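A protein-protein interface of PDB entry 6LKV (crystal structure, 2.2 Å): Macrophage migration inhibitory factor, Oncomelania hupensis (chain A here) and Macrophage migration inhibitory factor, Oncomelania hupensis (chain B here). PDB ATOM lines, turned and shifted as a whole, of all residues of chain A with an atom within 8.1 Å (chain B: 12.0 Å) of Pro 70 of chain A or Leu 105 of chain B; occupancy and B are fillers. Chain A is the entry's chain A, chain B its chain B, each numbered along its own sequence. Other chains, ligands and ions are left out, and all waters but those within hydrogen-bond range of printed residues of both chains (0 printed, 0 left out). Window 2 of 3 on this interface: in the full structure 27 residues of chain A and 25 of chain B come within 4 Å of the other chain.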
ATOM      1  N   ARG A  67      23.102  -9.651  15.213  1.00  0.00           N
ATOM      2  CA  ARG A  67      21.967  -9.281  16.092  1.00  0.00           C
ATOM      3  C   ARG A  67      21.830 -10.214  17.308  1.00  0.00           C
ATOM      4  O   ARG A  67      21.335  -9.725  18.332  1.00  0.00           O
ATOM      5  CB  ARG A  67      20.649  -9.274  15.319  1.00  0.00           C
ATOM      6  CG  ARG A  67      20.676  -8.505  14.021  1.00  0.00           C
ATOM      7  CD  ARG A  67      20.999  -7.038  14.261  1.00  0.00           C
ATOM      8  NE  ARG A  67      20.732  -6.233  13.069  1.00  0.00           N
ATOM      9  CZ  ARG A  67      21.621  -5.880  12.129  1.00  0.00           C
ATOM     10  NH1 ARG A  67      22.872  -6.251  12.203  1.00  0.00           N
ATOM     11  NH2 ARG A  67      21.225  -5.191  11.085  1.00  0.00           N
ATOM     12  N   LEU A  68      22.231 -11.481  17.214  1.00  0.00           N
ATOM     13  CA  LEU A  68      21.991 -12.472  18.298  1.00  0.00           C
ATOM     14  C   LEU A  68      23.159 -12.464  19.284  1.00  0.00           C
ATOM     15  O   LEU A  68      24.319 -12.701  18.857  1.00  0.00           O
ATOM     16  CB  LEU A  68      21.805 -13.865  17.687  1.00  0.00           C
ATOM     17  CG  LEU A  68      20.753 -13.971  16.576  1.00  0.00           C
ATOM     18  CD1 LEU A  68      20.622 -15.433  16.116  1.00  0.00           C
ATOM     19  CD2 LEU A  68      19.418 -13.422  17.035  1.00  0.00           C
ATOM     20  N   ASN A  69      22.839 -12.274  20.564  1.00  0.00           N
ATOM     21  CA  ASN A  69      23.801 -12.279  21.694  1.00  0.00           C
ATOM     22  C   ASN A  69      22.990 -12.579  22.952  1.00  0.00           C
ATOM     23  O   ASN A  69      21.759 -12.477  22.942  1.00  0.00           O
ATOM     24  CB  ASN A  69      24.559 -10.942  21.779  1.00  0.00           C
ATOM     25  CG  ASN A  69      23.648  -9.763  22.016  1.00  0.00           C
ATOM     26  OD1 ASN A  69      23.041  -9.653  23.065  1.00  0.00           O
ATOM     27  ND2 ASN A  69      23.477  -8.926  21.005  1.00  0.00           N
ATOM     28  N   PRO A  70      23.629 -12.959  24.073  1.00  0.00           N
ATOM     29  CA  PRO A  70      22.885 -13.356  25.271  1.00  0.00           C
ATOM     30  C   PRO A  70      21.832 -12.322  25.684  1.00  0.00           C
ATOM     31  O   PRO A  70      20.745 -12.739  26.109  1.00  0.00           O
ATOM     32  CB  PRO A  70      23.999 -13.521  26.319  1.00  0.00           C
ATOM     33  CG  PRO A  70      25.183 -13.979  25.490  1.00  0.00           C
ATOM     34  CD  PRO A  70      25.087 -13.133  24.231  1.00  0.00           C
ATOM     35  N   THR A  71      22.123 -11.023  25.522  1.00  0.00           N
ATOM     36  CA  THR A  71      21.206  -9.953  25.988  1.00  0.00           C
ATOM     37  C   THR A  71      19.998  -9.861  25.055  1.00  0.00           C
ATOM     38  O   THR A  71      18.866  -9.899  25.553  1.00  0.00           O
ATOM     39  CB  THR A  71      21.905  -8.590  26.142  1.00  0.00           C
ATOM     40  OG1 THR A  71      22.954  -8.742  27.097  1.00  0.00           O
ATOM     41  CG2 THR A  71      20.942  -7.546  26.652  1.00  0.00           C
ATOM     42  N   SER A  72      20.216  -9.697  23.754  1.00  0.00           N
ATOM     43  CA  SER A  72      19.121  -9.574  22.755  1.00  0.00           C
ATOM     44  C   SER A  72      18.294 -10.883  22.736  1.00  0.00           C
ATOM     45  O   SER A  72      17.077 -10.800  22.701  1.00  0.00           O
ATOM     46  CB  SER A  72      19.665  -9.193  21.386  1.00  0.00           C
ATOM     47  OG  SER A  72      20.473 -10.237  20.849  1.00  0.00           O
ATOM     48  N   ASN A  73      18.940 -12.038  22.887  1.00  0.00           N
ATOM     49  CA  ASN A  73      18.279 -13.373  22.846  1.00  0.00           C
ATOM     50  C   ASN A  73      17.225 -13.469  23.958  1.00  0.00           C
ATOM     51  O   ASN A  73      16.070 -13.847  23.660  1.00  0.00           O
ATOM     52  CB  ASN A  73      19.278 -14.511  22.970  1.00  0.00           C
ATOM     53  CG  ASN A  73      20.163 -14.654  21.762  1.00  0.00           C
ATOM     54  OD1 ASN A  73      19.925 -14.022  20.724  1.00  0.00           O
ATOM     55  ND2 ASN A  73      21.198 -15.464  21.905  1.00  0.00           N
ATOM     56  N   LEU A  74      17.586 -13.108  25.188  1.00  0.00           N
ATOM     57  CA  LEU A  74      16.658 -13.179  26.339  1.00  0.00           C
ATOM     58  C   LEU A  74      15.478 -12.236  26.106  1.00  0.00           C
ATOM     59  O   LEU A  74      14.314 -12.658  26.325  1.00  0.00           O
ATOM     60  CB  LEU A  74      17.394 -12.852  27.640  1.00  0.00           C
ATOM     61  CG  LEU A  74      16.523 -12.869  28.899  1.00  0.00           C
ATOM     62  CD1 LEU A  74      15.787 -14.195  29.050  1.00  0.00           C
ATOM     63  CD2 LEU A  74      17.374 -12.618  30.152  1.00  0.00           C
ATOM     64  N   ALA A  75      15.743 -10.999  25.686  1.00  0.00           N
ATOM     65  CA  ALA A  75      14.679  -9.994  25.496  1.00  0.00           C
ATOM     66  C   ALA A  75      13.720 -10.486  24.395  1.00  0.00           C
ATOM     67  O   ALA A  75      12.503 -10.396  24.582  1.00  0.00           O
ATOM     68  CB  ALA A  75      15.287  -8.644  25.163  1.00  0.00           C
ATOM     69  N   MET A  76      14.251 -10.990  23.288  1.00  0.00           N
ATOM     70  CA  MET A  76      13.426 -11.465  22.155  1.00  0.00           C
ATOM     71  C   MET A  76      12.643 -12.716  22.581  1.00  0.00           C
ATOM     72  O   MET A  76      11.454 -12.798  22.246  1.00  0.00           O
ATOM     73  CB  MET A  76      14.278 -11.758  20.912  1.00  0.00           C
ATOM     74  CG  MET A  76      14.740 -10.521  20.212  1.00  0.00           C
ATOM     75  SD  MET A  76      15.616 -10.900  18.665  1.00  0.00           S
ATOM     76  CE  MET A  76      17.139 -11.567  19.319  1.00  0.00           C
ATOM     77  N   ALA A  77      13.267 -13.618  23.338  1.00  0.00           N
ATOM     78  CA  ALA A  77      12.635 -14.858  23.869  1.00  0.00           C
ATOM     79  C   ALA A  77      11.384 -14.497  24.666  1.00  0.00           C
ATOM     80  O   ALA A  77      10.307 -15.082  24.407  1.00  0.00           O
ATOM     81  CB  ALA A  77      13.590 -15.653  24.698  1.00  0.00           C
ATOM     82  N   ILE A  97      12.872 -21.729  22.557  1.00  0.00           N
ATOM     83  CA  ILE A  97      13.294 -20.958  21.363  1.00  0.00           C
ATOM     84  C   ILE A  97      14.799 -21.137  21.207  1.00  0.00           C
ATOM     85  O   ILE A  97      15.521 -20.949  22.180  1.00  0.00           O
ATOM     86  CB  ILE A  97      12.889 -19.475  21.470  1.00  0.00           C
ATOM     87  CG1 ILE A  97      11.420 -19.328  21.822  1.00  0.00           C
ATOM     88  CG2 ILE A  97      13.267 -18.741  20.200  1.00  0.00           C
ATOM     89  CD1 ILE A  97      10.994 -17.929  22.210  1.00  0.00           C
ATOM     90  N   PHE A  99      18.074 -19.669  19.098  1.00  0.00           N
ATOM     91  CA  PHE A  99      18.641 -18.522  18.350  1.00  0.00           C
ATOM     92  C   PHE A  99      19.847 -19.061  17.595  1.00  0.00           C
ATOM     93  O   PHE A  99      20.736 -19.620  18.231  1.00  0.00           O
ATOM     94  CB  PHE A  99      18.940 -17.389  19.336  1.00  0.00           C
ATOM     95  CG  PHE A  99      17.704 -16.833  19.988  1.00  0.00           C
ATOM     96  CD1 PHE A  99      16.949 -15.843  19.385  1.00  0.00           C
ATOM     97  CD2 PHE A  99      17.286 -17.321  21.212  1.00  0.00           C
ATOM     98  CE1 PHE A  99      15.784 -15.385  19.990  1.00  0.00           C
ATOM     99  CE2 PHE A  99      16.126 -16.866  21.796  1.00  0.00           C
ATOM    100  CZ  PHE A  99      15.385 -15.881  21.202  1.00  0.00           C
ATOM    101  N   MET B   1      15.898 -27.069  22.606  1.00  0.00           N
ATOM    102  CA  MET B   1      16.610 -28.317  22.950  1.00  0.00           C
ATOM    103  C   MET B   1      16.025 -28.926  24.243  1.00  0.00           C
ATOM    104  O   MET B   1      15.422 -28.197  25.053  1.00  0.00           O
ATOM    105  CB  MET B   1      18.103 -27.998  23.083  1.00  0.00           C
ATOM    106  CG  MET B   1      18.487 -27.719  24.503  1.00  0.00           C
ATOM    107  SD  MET B   1      18.786 -29.225  25.487  1.00  0.00           S
ATOM    108  CE  MET B   1      18.417 -28.573  27.121  1.00  0.00           C
ATOM    109  N   LYS B  33      18.792 -35.611  30.203  1.00  0.00           N
ATOM    110  CA  LYS B  33      18.080 -34.328  30.326  1.00  0.00           C
ATOM    111  C   LYS B  33      16.743 -34.587  30.976  1.00  0.00           C
ATOM    112  O   LYS B  33      16.234 -35.687  30.901  1.00  0.00           O
ATOM    113  CB  LYS B  33      17.879 -33.717  28.927  1.00  0.00           C
ATOM    114  CG  LYS B  33      19.152 -33.237  28.258  1.00  0.00           C
ATOM    115  CD  LYS B  33      19.608 -31.927  28.873  1.00  0.00           C
ATOM    116  CE  LYS B  33      20.944 -31.479  28.337  1.00  0.00           C
ATOM    117  NZ  LYS B  33      20.963 -30.012  28.199  1.00  0.00           N
ATOM    118  N   CYS B  64      20.616 -30.233  21.132  1.00  0.00           N
ATOM    119  CA  CYS B  64      20.870 -30.437  22.565  1.00  0.00           C
ATOM    120  C   CYS B  64      21.967 -29.489  23.051  1.00  0.00           C
ATOM    121  O   CYS B  64      22.977 -29.303  22.333  1.00  0.00           O
ATOM    122  CB  CYS B  64      21.287 -31.890  22.791  1.00  0.00           C
ATOM    123  SG  CYS B  64      21.268 -32.318  24.549  1.00  0.00           S
ATOM    124  N   ILE B  65      21.797 -28.953  24.248  1.00  0.00           N
ATOM    125  CA  ILE B  65      22.848 -28.178  24.974  1.00  0.00           C
ATOM    126  C   ILE B  65      23.713 -29.200  25.709  1.00  0.00           C
ATOM    127  O   ILE B  65      23.162 -29.951  26.506  1.00  0.00           O
ATOM    128  CB  ILE B  65      22.216 -27.139  25.919  1.00  0.00           C
ATOM    129  CG1 ILE B  65      21.270 -26.210  25.169  1.00  0.00           C
ATOM    130  CG2 ILE B  65      23.282 -26.349  26.637  1.00  0.00           C
ATOM    131  CD1 ILE B  65      20.313 -25.429  26.039  1.00  0.00           C
ATOM    132  N   GLY B  66      25.009 -29.244  25.409  1.00  0.00           N
ATOM    133  CA  GLY B  66      25.920 -30.286  25.910  1.00  0.00           C
ATOM    134  C   GLY B  66      25.616 -31.648  25.300  1.00  0.00           C
ATOM    135  O   GLY B  66      24.877 -31.724  24.278  1.00  0.00           O
ATOM    136  N   ILE B 100      23.225 -31.623  16.646  1.00  0.00           N
ATOM    137  CA  ILE B 100      23.318 -30.146  16.578  1.00  0.00           C
ATOM    138  C   ILE B 100      23.579 -29.598  17.968  1.00  0.00           C
ATOM    139  O   ILE B 100      22.666 -29.508  18.790  1.00  0.00           O
ATOM    140  CB  ILE B 100      22.054 -29.515  15.958  1.00  0.00           C
ATOM    141  CG1 ILE B 100      21.700 -30.168  14.625  1.00  0.00           C
ATOM    142  CG2 ILE B 100      22.271 -28.026  15.819  1.00  0.00           C
ATOM    143  CD1 ILE B 100      20.513 -29.506  13.918  1.00  0.00           C
ATOM    144  N   PRO B 101      24.832 -29.193  18.262  1.00  0.00           N
ATOM    145  CA  PRO B 101      25.157 -28.550  19.528  1.00  0.00           C
ATOM    146  C   PRO B 101      24.475 -27.191  19.615  1.00  0.00           C
ATOM    147  O   PRO B 101      24.559 -26.447  18.689  1.00  0.00           O
ATOM    148  CB  PRO B 101      26.684 -28.332  19.497  1.00  0.00           C
ATOM    149  CG  PRO B 101      27.165 -29.292  18.458  1.00  0.00           C
ATOM    150  CD  PRO B 101      26.031 -29.410  17.444  1.00  0.00           C
ATOM    151  N   VAL B 102      23.806 -26.923  20.721  1.00  0.00           N
ATOM    152  CA  VAL B 102      23.080 -25.648  20.957  1.00  0.00           C
ATOM    153  C   VAL B 102      23.796 -24.908  22.093  1.00  0.00           C
ATOM    154  O   VAL B 102      24.072 -25.503  23.140  1.00  0.00           O
ATOM    155  CB  VAL B 102      21.604 -25.921  21.285  1.00  0.00           C
ATOM    156  CG1 VAL B 102      20.849 -24.658  21.599  1.00  0.00           C
ATOM    157  CG2 VAL B 102      20.908 -26.709  20.179  1.00  0.00           C
ATOM    158  N   PRO B 103      24.182 -23.621  21.912  1.00  0.00           N
ATOM    159  CA  PRO B 103      24.763 -22.840  23.003  1.00  0.00           C
ATOM    160  C   PRO B 103      23.711 -22.528  24.058  1.00  0.00           C
ATOM    161  O   PRO B 103      22.575 -22.154  23.687  1.00  0.00           O
ATOM    162  CB  PRO B 103      25.271 -21.535  22.366  1.00  0.00           C
ATOM    163  CG  PRO B 103      25.282 -21.845  20.857  1.00  0.00           C
ATOM    164  CD  PRO B 103      24.179 -22.872  20.645  1.00  0.00           C
ATOM    165  N   ALA B 104      24.101 -22.657  25.337  1.00  0.00           N
ATOM    166  CA  ALA B 104      23.238 -22.394  26.505  1.00  0.00           C
ATOM    167  C   ALA B 104      22.622 -20.994  26.445  1.00  0.00           C
ATOM    168  O   ALA B 104      21.435 -20.841  26.835  1.00  0.00           O
ATOM    169  CB  ALA B 104      24.044 -22.590  27.775  1.00  0.00           C
ATOM    170  N   LEU B 105      23.359 -19.997  25.959  1.00  0.00           N
ATOM    171  CA  LEU B 105      22.873 -18.586  25.961  1.00  0.00           C
ATOM    172  C   LEU B 105      22.198 -18.251  24.622  1.00  0.00           C
ATOM    173  O   LEU B 105      21.839 -17.080  24.440  1.00  0.00           O
ATOM    174  CB  LEU B 105      24.054 -17.644  26.249  1.00  0.00           C
ATOM    175  CG  LEU B 105      24.769 -17.875  27.580  1.00  0.00           C
ATOM    176  CD1 LEU B 105      25.934 -16.898  27.765  1.00  0.00           C
ATOM    177  CD2 LEU B 105      23.804 -17.754  28.734  1.00  0.00           C
ATOM    178  N   PHE B 106      21.997 -19.250  23.752  1.00  0.00           N
ATOM    179  CA  PHE B 106      21.306 -19.090  22.450  1.00  0.00           C
ATOM    180  C   PHE B 106      20.048 -19.972  22.430  1.00  0.00           C
ATOM    181  O   PHE B 106      19.567 -20.380  21.357  1.00  0.00           O
ATOM    182  CB  PHE B 106      22.292 -19.383  21.320  1.00  0.00           C
ATOM    183  CG  PHE B 106      23.233 -18.238  21.018  1.00  0.00           C
ATOM    184  CD1 PHE B 106      24.228 -17.872  21.916  1.00  0.00           C
ATOM    185  CD2 PHE B 106      23.094 -17.484  19.852  1.00  0.00           C
ATOM    186  CE1 PHE B 106      25.089 -16.809  21.630  1.00  0.00           C
ATOM    187  CE2 PHE B 106      23.942 -16.414  19.582  1.00  0.00           C
ATOM    188  CZ  PHE B 106      24.941 -16.077  20.469  1.00  0.00           C
ATOM    189  N   CYS B 107      19.509 -20.254  23.609  1.00  0.00           N
ATOM    190  CA  CYS B 107      18.317 -21.127  23.762  1.00  0.00           C
ATOM    191  C   CYS B 107      17.558 -20.738  25.026  1.00  0.00           C
ATOM    192  O   CYS B 107      18.171 -20.831  26.146  1.00  0.00           O
ATOM    193  CB  CYS B 107      18.693 -22.603  23.770  1.00  0.00           C
ATOM    194  SG  CYS B 107      17.239 -23.690  23.739  1.00  0.00           S
ATOM    195  N   SER B 108      16.301 -20.323  24.865  1.00  0.00           N
ATOM    196  CA  SER B 108      15.376 -19.988  25.971  1.00  0.00           C
ATOM    197  C   SER B 108      14.457 -21.176  26.308  1.00  0.00           C
ATOM    198  O   SER B 108      14.060 -21.933  25.412  1.00  0.00           O
ATOM    199  CB  SER B 108      14.601 -18.746  25.679  1.00  0.00           C
ATOM    200  OG  SER B 108      13.699 -18.900  24.597  1.00  0.00           O
ATOM    201  N   PHE B 109      14.165 -21.333  27.594  1.00  0.00           N
ATOM    202  CA  PHE B 109      13.092 -22.198  28.134  1.00  0.00           C
ATOM    203  C   PHE B 109      12.463 -21.437  29.287  1.00  0.00           C
ATOM    204  O   PHE B 109      13.199 -20.991  30.192  1.00  0.00           O
ATOM    205  CB  PHE B 109      13.593 -23.571  28.588  1.00  0.00           C
ATOM    206  CG  PHE B 109      12.606 -24.311  29.451  1.00  0.00           C
ATOM    207  CD1 PHE B 109      11.337 -24.604  28.968  1.00  0.00           C
ATOM    208  CD2 PHE B 109      12.909 -24.656  30.766  1.00  0.00           C
ATOM    209  CE1 PHE B 109      10.402 -25.260  29.760  1.00  0.00           C
ATOM    210  CE2 PHE B 109      11.985 -25.329  31.561  1.00  0.00           C
ATOM    211  CZ  PHE B 109      10.729 -25.618  31.062  1.00  0.00           C
ATOM    212  N   GLY B 111      11.194 -18.491  29.973  1.00  0.00           N
ATOM    213  CA  GLY B 111      11.457 -17.090  30.373  1.00  0.00           C
ATOM    214  C   GLY B 111      12.924 -16.841  30.697  1.00  0.00           C
ATOM    215  O   GLY B 111      13.247 -15.703  31.065  1.00  0.00           O
ATOM    216  N   ALA B 112      13.806 -17.823  30.503  1.00  0.00           N
ATOM    217  CA  ALA B 112      15.248 -17.688  30.824  1.00  0.00           C
ATOM    218  C   ALA B 112      16.105 -18.431  29.799  1.00  0.00           C
ATOM    219  O   ALA B 112      15.603 -19.356  29.129  1.00  0.00           O
ATOM    220  CB  ALA B 112      15.516 -18.212  32.233  1.00  0.00           C
ATOM    221  N   LEU B 113      17.383 -18.090  29.734  1.00  0.00           N
ATOM    222  CA  LEU B 113      18.379 -18.862  28.961  1.00  0.00           C
ATOM    223  C   LEU B 113      18.801 -20.057  29.814  1.00  0.00           C
ATOM    224  O   LEU B 113      18.143 -20.328  30.797  1.00  0.00           O
ATOM    225  CB  LEU B 113      19.561 -17.963  28.574  1.00  0.00           C
ATOM    226  CG  LEU B 113      19.193 -16.652  27.881  1.00  0.00           C
ATOM    227  CD1 LEU B 113      20.454 -15.899  27.515  1.00  0.00           C
ATOM    228  CD2 LEU B 113      18.355 -16.889  26.637  1.00  0.00           C
ATOM    229  N   HIS B 114      19.832 -20.772  29.394  1.00  0.00           N
ATOM    230  CA  HIS B 114      20.334 -21.980  30.082  1.00  0.00           C
ATOM    231  C   HIS B 114      21.722 -21.698  30.675  1.00  0.00           C
ATOM    232  O   HIS B 114      22.395 -20.746  30.218  1.00  0.00           O
ATOM    233  CB  HIS B 114      20.365 -23.150  29.092  1.00  0.00           C
ATOM    234  CG  HIS B 114      19.023 -23.634  28.686  1.00  0.00           C
ATOM    235  ND1 HIS B 114      18.260 -22.974  27.733  1.00  0.00           N
ATOM    236  CD2 HIS B 114      18.318 -24.716  29.067  1.00  0.00           C
ATOM    237  CE1 HIS B 114      17.131 -23.626  27.553  1.00  0.00           C
ATOM    238  NE2 HIS B 114      17.142 -24.706  28.365  1.00  0.00           N
ATOM    239  N   ASP B 115      22.142 -22.556  31.597  1.00  0.00           N
ATOM    240  CA  ASP B 115      23.461 -22.496  32.271  1.00  0.00           C
ATOM    241  C   ASP B 115      24.537 -22.936  31.284  1.00  0.00           C
ATOM    242  O   ASP B 115      24.451 -24.085  30.750  1.00  0.00           O
ATOM    243  CB  ASP B 115      23.455 -23.409  33.505  1.00  0.00           C
ATOM    244  CG  ASP B 115      23.866 -22.741  34.801  1.00  0.00           C
ATOM    245  OD1 ASP B 115      24.607 -21.718  34.746  1.00  0.00           O
ATOM    246  OD2 ASP B 115      23.418 -23.245  35.849  1.00  0.00           O
ATOM    247  N   VAL B 116      25.560 -22.106  31.090  1.00  0.00           N
ATOM    248  CA  VAL B 116      26.720 -22.371  30.182  1.00  0.00           C
ATOM    249  C   VAL B 116      27.463 -23.647  30.636  1.00  0.00           C
ATOM    250  O   VAL B 116      28.111 -24.303  29.781  1.00  0.00           O
ATOM    251  CB  VAL B 116      27.653 -21.146  30.106  1.00  0.00           C
ATOM    252  CG1 VAL B 116      28.297 -20.829  31.462  1.00  0.00           C
ATOM    253  CG2 VAL B 116      28.714 -21.315  29.020  1.00  0.00           C
ATOM    254  N   SER B 117      27.410 -23.992  31.921  1.00  0.00           N
ATOM    255  CA  SER B 117      28.162 -25.160  32.466  1.00  0.00           C
ATOM    256  C   SER B 117      27.635 -26.463  31.821  1.00  0.00           C
ATOM    257  O   SER B 117      28.427 -27.449  31.642  1.00  0.00           O
ATOM    258  CB  SER B 117      28.106 -25.214  33.966  1.00  0.00           C
ATOM    259  OG  SER B 117      26.767 -25.242  34.415  1.00  0.00           O
ATOM    260  N   ILE B 118      26.358 -26.475  31.429  1.00  0.00           N
ATOM    261  CA  ILE B 118      25.719 -27.659  30.779  1.00  0.00           C
ATOM    262  C   ILE B 118      26.416 -27.952  29.450  1.00  0.00           C
ATOM    263  O   ILE B 118      26.546 -29.148  29.125  1.00  0.00           O
ATOM    264  CB  ILE B 118      24.212 -27.447  30.639  1.00  0.00           C
ATOM    265  CG1 ILE B 118      23.562 -27.291  32.016  1.00  0.00           C
ATOM    266  CG2 ILE B 118      23.576 -28.584  29.861  1.00  0.00           C
ATOM    267  CD1 ILE B 118      22.263 -26.547  31.963  1.00  0.00           C
ATOM    268  N   GLU B 119      26.928 -26.941  28.748  1.00  0.00           N
ATOM    269  CA  GLU B 119      27.570 -27.131  27.425  1.00  0.00           C
ATOM    270  C   GLU B 119      28.734 -28.097  27.531  1.00  0.00           C
ATOM    271  O   GLU B 119      28.995 -28.804  26.527  1.00  0.00           O
ATOM    272  CB  GLU B 119      28.119 -25.837  26.824  1.00  0.00           C
ATOM    273  CG  GLU B 119      27.056 -24.908  26.305  1.00  0.00           C
ATOM    274  CD  GLU B 119      27.658 -23.635  25.734  1.00  0.00           C
ATOM    275  OE1 GLU B 119      28.860 -23.633  25.411  1.00  0.00           O
ATOM    276  OE2 GLU B 119      26.913 -22.671  25.552  1.00  0.00           O
ATOM    277  N   ARG B 120      29.437 -28.086  28.661  1.00  0.00           N
ATOM    278  CA  ARG B 120      30.636 -28.932  28.900  1.00  0.00           C
ATOM    279  C   ARG B 120      30.257 -30.111  29.809  1.00  0.00           C
ATOM    280  O   ARG B 120      31.182 -30.810  30.287  1.00  0.00           O
ATOM    281  CB  ARG B 120      31.771 -28.093  29.506  1.00  0.00           C
ATOM    282  CG  ARG B 120      32.380 -27.060  28.565  1.00  0.00           C
ATOM    283  CD  ARG B 120      33.486 -26.208  29.209  1.00  0.00           C
ATOM    284  NE  ARG B 120      33.078 -25.528  30.444  1.00  0.00           N
ATOM    285  CZ  ARG B 120      32.304 -24.433  30.514  1.00  0.00           C
ATOM    286  NH1 ARG B 120      31.829 -23.867  29.418  1.00  0.00           N
ATOM    287  NH2 ARG B 120      31.991 -23.908  31.691  1.00  0.00           N
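Printed residues of chain A that touch a printed residue of chain B: Leu 68, Pro 70, Asn 73, Leu 74, Ala 77, Ile 97 and Phe 99.
Hydrophobic or aromatic side chains of chain A that line the printed part of chain B: Leu 68, Pro 70, Leu 74, Ala 77, Ile 97 and Phe 99.
Among the printed residues, 11 pairs touch across the chains.
Printed residues of chain B within 4 Å of Pro 70 of chain A: Leu 105 (3.8 Å) and Leu 113 (3.5 Å).
Of chain A, only Pro 70 (3.8 Å) and Asn 73 (3.1 Å) come within 4 Å of Leu 105 of chain B.
No residue of chain B comes within 4 Å of Asn 69 of chain A.
No residue of chain B comes within 4 Å of Thr 71 of chain A.
Asn 73 of chain A touches just these residues of chain B: Leu 105 (3.1 Å) and Phe 106 (3.4 Å).
Printed residues of chain A within 4 Å of Leu 113 of chain B: Pro 70.
Of the printed residues of chain B, Ala 77 of chain A touches Ser 108 (3.3 Å).
Printed residues of chain A within 4 Å of Phe 106 of chain B: Leu 68 (3.8 Å), Asn 73 (3.4 Å) and Phe 99 (2.8 Å).
Of the printed residues of chain B, Ile 97 of chain A touches Cys 107 and Ser 108.
Ala 75 of chain A touches none of the printed residues of chain B.
The nearest printed residue of chain B that does not touch Leu 68 of chain A is Leu 105 of chain B (7.0 Å).
ND2 of Asn 73 of chain A sits close to O of Asn 69 of chain A (3.2 Å).
A ring nitrogen (ND1) of His 114 of chain B is in hydrogen-bond range of the backbone carbonyl oxygen of Cys 107 of chain B (2.7 Å).
Phe 106 of chain B touches Leu 68 of chain A (CZ to O, 3.8 Å).
Pro 70 of chain A touches Leu 105 of chain B (CG to CD1, 3.8 Å).
Leu 113 of chain B touches Pro 70 of chain A (CD1 to O, 3.5 Å).
Asn 73 of chain A touches Phe 106 of chain B (ND2 to CD2, 3.4 Å).
Gly 111 of chain B touches Leu 74 of chain A (O to CD1, 3.6 Å).
Leu 74 of chain A touches Ala 112 of chain B (CD1 to CA, 3.95 Å).
OG of Ser 108 of chain B touches CB of Ala 77 of chain A, at 3.3 Å.
O of Ile 97 of chain A sits close to SG of Cys 107 of chain B.
The backbone carbonyl oxygen of Phe 106 of chain B lies within hydrogen-bond range of the backbone NH of Phe 99 of chain A, 2.8 Å away.
The backbone NH (N) of Ser 108 of chain B sits at hydrogen-bond distance from the backbone carbonyl oxygen (O) of Ile 97 of chain A, 2.9 Å away.
The side-chain amide nitrogen (ND2) of Asn 73 of chain A is in hydrogen-bond range of the backbone carbonyl oxygen (O) of Leu 105 of chain B (3.1 Å).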
